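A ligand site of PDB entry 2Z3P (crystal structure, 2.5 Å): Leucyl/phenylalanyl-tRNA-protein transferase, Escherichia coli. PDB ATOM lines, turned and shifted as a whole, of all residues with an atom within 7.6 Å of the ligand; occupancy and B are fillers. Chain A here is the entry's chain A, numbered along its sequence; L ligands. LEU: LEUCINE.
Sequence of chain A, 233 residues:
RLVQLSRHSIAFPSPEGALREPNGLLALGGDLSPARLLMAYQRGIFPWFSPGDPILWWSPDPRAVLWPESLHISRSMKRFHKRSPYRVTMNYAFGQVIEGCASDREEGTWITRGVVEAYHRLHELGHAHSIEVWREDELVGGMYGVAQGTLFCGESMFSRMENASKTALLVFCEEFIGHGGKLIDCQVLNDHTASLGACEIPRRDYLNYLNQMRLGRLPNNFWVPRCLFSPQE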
ATOM      1  N   ALA A  64     -26.753   0.368   8.597  1.00  0.00           N
ATOM      2  CA  ALA A  64     -26.912   1.817   8.607  1.00  0.00           C
ATOM      3  C   ALA A  64     -25.788   2.435   7.783  1.00  0.00           C
ATOM      4  O   ALA A  64     -24.622   2.084   7.945  1.00  0.00           O
ATOM      5  CB  ALA A  64     -26.902   2.356  10.037  1.00  0.00           C
ATOM      6  N   VAL A  65     -26.130   3.372   6.910  1.00  0.00           N
ATOM      7  CA  VAL A  65     -25.099   3.976   6.082  1.00  0.00           C
ATOM      8  C   VAL A  65     -25.310   5.474   5.857  1.00  0.00           C
ATOM      9  O   VAL A  65     -26.392   6.024   6.097  1.00  0.00           O
ATOM     10  CB  VAL A  65     -25.021   3.216   4.728  1.00  0.00           C
ATOM     11  CG1 VAL A  65     -25.740   3.978   3.636  1.00  0.00           C
ATOM     12  CG2 VAL A  65     -23.593   2.950   4.367  1.00  0.00           C
ATOM     13  N   LEU A  66     -24.254   6.152   5.411  1.00  0.00           N
ATOM     14  CA  LEU A  66     -24.343   7.596   5.155  1.00  0.00           C
ATOM     15  C   LEU A  66     -23.698   8.021   3.846  1.00  0.00           C
ATOM     16  O   LEU A  66     -22.470   7.978   3.683  1.00  0.00           O
ATOM     17  CB  LEU A  66     -23.687   8.368   6.311  1.00  0.00           C
ATOM     18  CG  LEU A  66     -23.497   9.889   6.118  1.00  0.00           C
ATOM     19  CD1 LEU A  66     -24.839  10.541   5.825  1.00  0.00           C
ATOM     20  CD2 LEU A  66     -22.859  10.494   7.378  1.00  0.00           C
ATOM     21  N   CYS A 101     -14.030   8.530  22.841  1.00  0.00           N
ATOM     22  CA  CYS A 101     -15.250   7.793  22.565  1.00  0.00           C
ATOM     23  C   CYS A 101     -15.478   6.794  23.689  1.00  0.00           C
ATOM     24  O   CYS A 101     -16.612   6.543  24.089  1.00  0.00           O
ATOM     25  CB  CYS A 101     -15.152   7.084  21.227  1.00  0.00           C
ATOM     26  SG  CYS A 101     -15.051   8.185  19.790  1.00  0.00           S
ATOM     27  N   GLY A 142     -14.413  14.500  17.822  1.00  0.00           N
ATOM     28  CA  GLY A 142     -13.786  13.778  16.748  1.00  0.00           C
ATOM     29  C   GLY A 142     -14.501  12.485  16.464  1.00  0.00           C
ATOM     30  O   GLY A 142     -15.595  12.229  16.968  1.00  0.00           O
ATOM     31  N   MET A 143     -13.880  11.659  15.634  1.00  0.00           N
ATOM     32  CA  MET A 143     -14.422  10.367  15.269  1.00  0.00           C
ATOM     33  C   MET A 143     -13.265   9.523  14.701  1.00  0.00           C
ATOM     34  O   MET A 143     -12.247  10.063  14.261  1.00  0.00           O
ATOM     35  CB  MET A 143     -15.506  10.519  14.199  1.00  0.00           C
ATOM     36  CG  MET A 143     -14.978  10.752  12.788  1.00  0.00           C
ATOM     37  SD  MET A 143     -16.111  10.187  11.472  1.00  0.00           S
ATOM     38  CE  MET A 143     -16.196  11.649  10.464  1.00  0.00           C
ATOM     39  N   TYR A 144     -13.435   8.211  14.728  1.00  0.00           N
ATOM     40  CA  TYR A 144     -12.393   7.350  14.191  1.00  0.00           C
ATOM     41  C   TYR A 144     -13.046   6.182  13.490  1.00  0.00           C
ATOM     42  O   TYR A 144     -14.190   5.833  13.790  1.00  0.00           O
ATOM     43  CB  TYR A 144     -11.483   6.837  15.290  1.00  0.00           C
ATOM     44  CG  TYR A 144     -12.115   5.788  16.180  1.00  0.00           C
ATOM     45  CD1 TYR A 144     -13.030   6.148  17.172  1.00  0.00           C
ATOM     46  CD2 TYR A 144     -11.778   4.447  16.048  1.00  0.00           C
ATOM     47  CE1 TYR A 144     -13.583   5.184  18.018  1.00  0.00           C
ATOM     48  CE2 TYR A 144     -12.325   3.477  16.882  1.00  0.00           C
ATOM     49  CZ  TYR A 144     -13.221   3.846  17.861  1.00  0.00           C
ATOM     50  OH  TYR A 144     -13.757   2.890  18.683  1.00  0.00           O
ATOM     51  N   GLY A 145     -12.332   5.578  12.553  1.00  0.00           N
ATOM     52  CA  GLY A 145     -12.874   4.433  11.844  1.00  0.00           C
ATOM     53  C   GLY A 145     -11.859   3.659  11.026  1.00  0.00           C
ATOM     54  O   GLY A 145     -10.664   3.958  11.042  1.00  0.00           O
ATOM     55  N   PHE A 152     -15.720   4.082   3.964  1.00  0.00           N
ATOM     56  CA  PHE A 152     -15.167   4.361   5.289  1.00  0.00           C
ATOM     57  C   PHE A 152     -16.141   3.885   6.341  1.00  0.00           C
ATOM     58  O   PHE A 152     -17.341   4.232   6.307  1.00  0.00           O
ATOM     59  CB  PHE A 152     -14.879   5.856   5.485  1.00  0.00           C
ATOM     60  CG  PHE A 152     -14.195   6.166   6.788  1.00  0.00           C
ATOM     61  CD1 PHE A 152     -12.867   5.827   6.983  1.00  0.00           C
ATOM     62  CD2 PHE A 152     -14.909   6.733   7.837  1.00  0.00           C
ATOM     63  CE1 PHE A 152     -12.247   6.062   8.215  1.00  0.00           C
ATOM     64  CE2 PHE A 152     -14.294   6.974   9.080  1.00  0.00           C
ATOM     65  CZ  PHE A 152     -12.969   6.636   9.255  1.00  0.00           C
ATOM     66  N   CYS A 153     -15.655   3.058   7.260  1.00  0.00           N
ATOM     67  CA  CYS A 153     -16.479   2.538   8.326  1.00  0.00           C
ATOM     68  C   CYS A 153     -16.250   3.416   9.556  1.00  0.00           C
ATOM     69  O   CYS A 153     -15.187   3.377  10.184  1.00  0.00           O
ATOM     70  CB  CYS A 153     -16.091   1.088   8.642  1.00  0.00           C
ATOM     71  SG  CYS A 153     -16.202  -0.013   7.198  1.00  0.00           S
ATOM     72  N   GLY A 154     -17.263   4.233   9.866  1.00  0.00           N
ATOM     73  CA  GLY A 154     -17.157   5.111  11.006  1.00  0.00           C
ATOM     74  C   GLY A 154     -17.455   4.289  12.224  1.00  0.00           C
ATOM     75  O   GLY A 154     -18.569   3.788  12.376  1.00  0.00           O
ATOM     76  N   GLU A 155     -16.476   4.146  13.109  1.00  0.00           N
ATOM     77  CA  GLU A 155     -16.648   3.362  14.325  1.00  0.00           C
ATOM     78  C   GLU A 155     -17.423   4.101  15.385  1.00  0.00           C
ATOM     79  O   GLU A 155     -18.369   3.572  15.954  1.00  0.00           O
ATOM     80  CB  GLU A 155     -15.283   2.964  14.869  1.00  0.00           C
ATOM     81  CG  GLU A 155     -14.669   1.803  14.131  1.00  0.00           C
ATOM     82  CD  GLU A 155     -15.365   0.503  14.452  1.00  0.00           C
ATOM     83  OE1 GLU A 155     -15.220   0.049  15.614  1.00  0.00           O
ATOM     84  OE2 GLU A 155     -16.057  -0.056  13.567  1.00  0.00           O
ATOM     85  N   SER A 156     -17.028   5.334  15.663  1.00  0.00           N
ATOM     86  CA  SER A 156     -17.695   6.132  16.674  1.00  0.00           C
ATOM     87  C   SER A 156     -17.258   7.585  16.631  1.00  0.00           C
ATOM     88  O   SER A 156     -16.350   7.951  15.895  1.00  0.00           O
ATOM     89  CB  SER A 156     -17.393   5.538  18.051  1.00  0.00           C
ATOM     90  OG  SER A 156     -18.200   6.148  19.035  1.00  0.00           O
ATOM     91  N   MET A 157     -17.926   8.429  17.408  1.00  0.00           N
ATOM     92  CA  MET A 157     -17.572   9.839  17.491  1.00  0.00           C
ATOM     93  C   MET A 157     -17.961  10.376  18.859  1.00  0.00           C
ATOM     94  O   MET A 157     -18.703   9.725  19.585  1.00  0.00           O
ATOM     95  CB  MET A 157     -18.216  10.650  16.356  1.00  0.00           C
ATOM     96  CG  MET A 157     -19.710  10.690  16.311  1.00  0.00           C
ATOM     97  SD  MET A 157     -20.235  11.600  14.831  1.00  0.00           S
ATOM     98  CE  MET A 157     -21.788  10.817  14.480  1.00  0.00           C
ATOM     99  N   PHE A 158     -17.429  11.533  19.225  1.00  0.00           N
ATOM    100  CA  PHE A 158     -17.708  12.101  20.533  1.00  0.00           C
ATOM    101  C   PHE A 158     -17.635  13.618  20.543  1.00  0.00           C
ATOM    102  O   PHE A 158     -16.975  14.242  19.698  1.00  0.00           O
ATOM    103  CB  PHE A 158     -16.719  11.524  21.568  1.00  0.00           C
ATOM    104  CG  PHE A 158     -15.369  12.190  21.567  1.00  0.00           C
ATOM    105  CD1 PHE A 158     -15.005  13.083  22.582  1.00  0.00           C
ATOM    106  CD2 PHE A 158     -14.437  11.931  20.552  1.00  0.00           C
ATOM    107  CE1 PHE A 158     -13.757  13.705  22.599  1.00  0.00           C
ATOM    108  CE2 PHE A 158     -13.170  12.548  20.546  1.00  0.00           C
ATOM    109  CZ  PHE A 158     -12.833  13.438  21.575  1.00  0.00           C
ATOM    110  N   LEU A 169     -17.641  15.560  11.301  1.00  0.00           N
ATOM    111  CA  LEU A 169     -18.222  14.836  10.192  1.00  0.00           C
ATOM    112  C   LEU A 169     -18.450  15.731   8.965  1.00  0.00           C
ATOM    113  O   LEU A 169     -18.279  15.279   7.828  1.00  0.00           O
ATOM    114  CB  LEU A 169     -19.538  14.194  10.644  1.00  0.00           C
ATOM    115  CG  LEU A 169     -20.202  13.228   9.651  1.00  0.00           C
ATOM    116  CD1 LEU A 169     -19.247  12.088   9.311  1.00  0.00           C
ATOM    117  CD2 LEU A 169     -21.498  12.699  10.271  1.00  0.00           C
ATOM    118  N   ILE A 184     -20.072   6.023   3.729  1.00  0.00           N
ATOM    119  CA  ILE A 184     -19.694   5.946   5.125  1.00  0.00           C
ATOM    120  C   ILE A 184     -20.563   4.889   5.762  1.00  0.00           C
ATOM    121  O   ILE A 184     -21.782   4.966   5.659  1.00  0.00           O
ATOM    122  CB  ILE A 184     -19.982   7.237   5.929  1.00  0.00           C
ATOM    123  CG1 ILE A 184     -19.077   8.379   5.458  1.00  0.00           C
ATOM    124  CG2 ILE A 184     -19.781   6.968   7.416  1.00  0.00           C
ATOM    125  CD1 ILE A 184     -17.653   7.973   5.464  1.00  0.00           C
ATOM    126  N   ASP A 185     -19.961   3.898   6.406  1.00  0.00           N
ATOM    127  CA  ASP A 185     -20.748   2.869   7.070  1.00  0.00           C
ATOM    128  C   ASP A 185     -20.994   3.360   8.494  1.00  0.00           C
ATOM    129  O   ASP A 185     -20.068   3.883   9.135  1.00  0.00           O
ATOM    130  CB  ASP A 185     -19.970   1.532   7.074  1.00  0.00           C
ATOM    131  CG  ASP A 185     -20.539   0.522   8.054  1.00  0.00           C
ATOM    132  OD1 ASP A 185     -21.774   0.389   8.137  1.00  0.00           O
ATOM    133  OD2 ASP A 185     -19.747  -0.150   8.738  1.00  0.00           O
ATOM    134  N   CYS A 186     -22.231   3.206   8.972  1.00  0.00           N
ATOM    135  CA  CYS A 186     -22.576   3.626  10.332  1.00  0.00           C
ATOM    136  C   CYS A 186     -23.035   2.470  11.212  1.00  0.00           C
ATOM    137  O   CYS A 186     -23.369   2.696  12.377  1.00  0.00           O
ATOM    138  CB  CYS A 186     -23.684   4.675  10.324  1.00  0.00           C
ATOM    139  SG  CYS A 186     -23.325   6.151   9.350  1.00  0.00           S
ATOM    140  N   GLN A 187     -23.040   1.265  10.663  1.00  0.00           N
ATOM    141  CA  GLN A 187     -23.458   0.037  11.373  1.00  0.00           C
ATOM    142  C   GLN A 187     -24.920   0.009  11.769  1.00  0.00           C
ATOM    143  O   GLN A 187     -25.748  -0.591  11.080  1.00  0.00           O
ATOM    144  CB  GLN A 187     -22.629  -0.187  12.639  1.00  0.00           C
ATOM    145  CG  GLN A 187     -21.127  -0.187  12.459  1.00  0.00           C
ATOM    146  CD  GLN A 187     -20.477   0.974  13.180  1.00  0.00           C
ATOM    147  OE1 GLN A 187     -20.119   1.962  12.551  1.00  0.00           O
ATOM    148  NE2 GLN A 187     -20.315   0.859  14.512  1.00  0.00           N
ATOM    149  N   VAL A 188     -25.252   0.633  12.884  1.00  0.00           N
ATOM    150  CA  VAL A 188     -26.636   0.667  13.348  1.00  0.00           C
ATOM    151  C   VAL A 188     -27.132   2.086  13.558  1.00  0.00           C
ATOM    152  O   VAL A 188     -26.551   2.864  14.321  1.00  0.00           O
ATOM    153  CB  VAL A 188     -26.781  -0.124  14.671  1.00  0.00           C
ATOM    154  CG1 VAL A 188     -28.228  -0.046  15.166  1.00  0.00           C
ATOM    155  CG2 VAL A 188     -26.356  -1.577  14.452  1.00  0.00           C
ATOM    156  N   LEU A 189     -28.212   2.423  12.884  1.00  0.00           N
ATOM    157  CA  LEU A 189     -28.803   3.745  12.958  1.00  0.00           C
ATOM    158  C   LEU A 189     -29.206   4.145  14.389  1.00  0.00           C
ATOM    159  O   LEU A 189     -29.573   3.310  15.203  1.00  0.00           O
ATOM    160  CB  LEU A 189     -30.026   3.770  12.024  1.00  0.00           C
ATOM    161  CG  LEU A 189     -30.653   5.076  11.506  1.00  0.00           C
ATOM    162  CD1 LEU A 189     -31.366   5.762  12.656  1.00  0.00           C
ATOM    163  CD2 LEU A 189     -29.595   5.977  10.887  1.00  0.00           C
ATOM    164  N   ASN A 190     -29.077   5.435  14.694  1.00  0.00           N
ATOM    165  CA  ASN A 190     -29.463   5.973  16.000  1.00  0.00           C
ATOM    166  C   ASN A 190     -29.859   7.435  15.807  1.00  0.00           C
ATOM    167  O   ASN A 190     -29.231   8.149  15.029  1.00  0.00           O
ATOM    168  CB  ASN A 190     -28.311   5.849  17.017  1.00  0.00           C
ATOM    169  CG  ASN A 190     -27.133   6.741  16.672  1.00  0.00           C
ATOM    170  OD1 ASN A 190     -27.256   7.967  16.614  1.00  0.00           O
ATOM    171  ND2 ASN A 190     -25.959   6.120  16.467  1.00  0.00           N
ATOM    172  N   HIS A 192     -29.268  10.415  16.491  1.00  0.00           N
ATOM    173  CA  HIS A 192     -28.303  11.419  16.051  1.00  0.00           C
ATOM    174  C   HIS A 192     -27.817  11.159  14.626  1.00  0.00           C
ATOM    175  O   HIS A 192     -27.863  12.062  13.783  1.00  0.00           O
ATOM    176  CB  HIS A 192     -27.081  11.472  16.975  1.00  0.00           C
ATOM    177  CG  HIS A 192     -26.190  12.645  16.721  1.00  0.00           C
ATOM    178  ND1 HIS A 192     -24.908  12.745  17.229  1.00  0.00           N
ATOM    179  CD2 HIS A 192     -26.385  13.783  16.005  1.00  0.00           C
ATOM    180  CE1 HIS A 192     -24.362  13.886  16.841  1.00  0.00           C
ATOM    181  NE2 HIS A 192     -25.243  14.531  16.092  1.00  0.00           N
ATOM    182  N   THR A 193     -27.354   9.944  14.361  1.00  0.00           N
ATOM    183  CA  THR A 193     -26.859   9.613  13.036  1.00  0.00           C
ATOM    184  C   THR A 193     -27.981   9.775  12.003  1.00  0.00           C
ATOM    185  O   THR A 193     -27.743  10.187  10.866  1.00  0.00           O
ATOM    186  CB  THR A 193     -26.270   8.156  13.012  1.00  0.00           C
ATOM    187  OG1 THR A 193     -25.473   7.973  11.838  1.00  0.00           O
ATOM    188  CG2 THR A 193     -27.370   7.098  13.029  1.00  0.00           C
ATOM    189  N   LEU A 196     -28.448  13.301  10.953  1.00  0.00           N
ATOM    190  CA  LEU A 196     -27.344  13.734  10.092  1.00  0.00           C
ATOM    191  C   LEU A 196     -27.512  13.261   8.659  1.00  0.00           C
ATOM    192  O   LEU A 196     -26.678  13.552   7.794  1.00  0.00           O
ATOM    193  CB  LEU A 196     -26.003  13.256  10.670  1.00  0.00           C
ATOM    194  CG  LEU A 196     -25.506  14.064  11.874  1.00  0.00           C
ATOM    195  CD1 LEU A 196     -24.243  13.452  12.435  1.00  0.00           C
ATOM    196  CD2 LEU A 196     -25.266  15.522  11.449  1.00  0.00           C
ATOM    197  N   ALA A 198     -28.138   9.847   7.859  1.00  0.00           N
ATOM    198  CA  ALA A 198     -27.797   8.444   7.675  1.00  0.00           C
ATOM    199  C   ALA A 198     -29.105   7.715   7.394  1.00  0.00           C
ATOM    200  O   ALA A 198     -30.169   8.179   7.783  1.00  0.00           O
ATOM    201  CB  ALA A 198     -27.115   7.882   8.936  1.00  0.00           C
HETATM  202  N   LEU L   1     -21.021   4.175  13.981  1.00  0.00           N
HETATM  203  CA  LEU L   1     -20.736   5.643  14.066  1.00  0.00           C
HETATM  204  C   LEU L   1     -21.670   6.335  15.061  1.00  0.00           C
HETATM  205  O   LEU L   1     -21.166   7.192  15.838  1.00  0.00           O
HETATM  206  CB  LEU L   1     -20.906   6.310  12.695  1.00  0.00           C
HETATM  207  CG  LEU L   1     -20.688   7.838  12.711  1.00  0.00           C
HETATM  208  CD1 LEU L   1     -19.237   8.130  13.078  1.00  0.00           C
HETATM  209  CD2 LEU L   1     -21.025   8.449  11.349  1.00  0.00           C
HETATM  210  OXT LEU L   1     -22.887   6.041  15.049  1.00  0.00           O
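A nitrogen (N) of the ligand sits at hydrogen-bond distance from the backbone carbonyl oxygen (O) of Gly 154 (3.0 Å).
OE1 of Gln 187 is in hydrogen-bond range of N of the ligand, 2.8 Å away.
The backbone carbonyl oxygen of Cys 186 is in hydrogen-bond range of a nitrogen (N) of the ligand, 3.2 Å away.
The backbone carbonyl oxygen (O) of Glu 155 is in hydrogen-bond range of a nitrogen (N) of the ligand (3.4 Å).
OXT of the ligand is in hydrogen-bond range of ND2 of Asn 190, 3.4 Å away.
O of Ala 64 is in hydrogen-bond range of N of Cys 186 (2.8 Å).
The backbone NH (N) of Glu 155 is in hydrogen-bond range of the backbone carbonyl oxygen (O) of Tyr 144 (2.9 Å).
The side-chain sulfur (SG) of Cys 186 sits at hydrogen-bond distance from the side-chain hydroxyl (OG1) of Thr 193 (3.8 Å).
The backbone NH (N) of Gly 154 lies within hydrogen-bond range of the backbone carbonyl oxygen (O) of Asp 185 (2.9 Å).
O of Ser 156 is in hydrogen-bond range of N of Tyr 144, 3.2 Å away.
The side-chain amide oxygen (OE1) of Gln 187 lies close to the backbone carbonyl oxygen (O) of Gly 154, at 2.4 Å.
The backbone NH (N) of Gln 187 is in hydrogen-bond range of the side-chain carboxylate (OD1) of Asp 185 (3.0 Å).
OD1 of Asn 190 sits at hydrogen-bond distance from N of Thr 193 (3.0 Å).
Merely in contact with the ligand: Ser 156 (3.7 Å) and Met 157 (3.6 Å).
Of the 27 residues printed, 7 come within 4 Å of the ligand.
The nearest printed residue that does not touch the ligand is Met 143 (4.1 Å).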
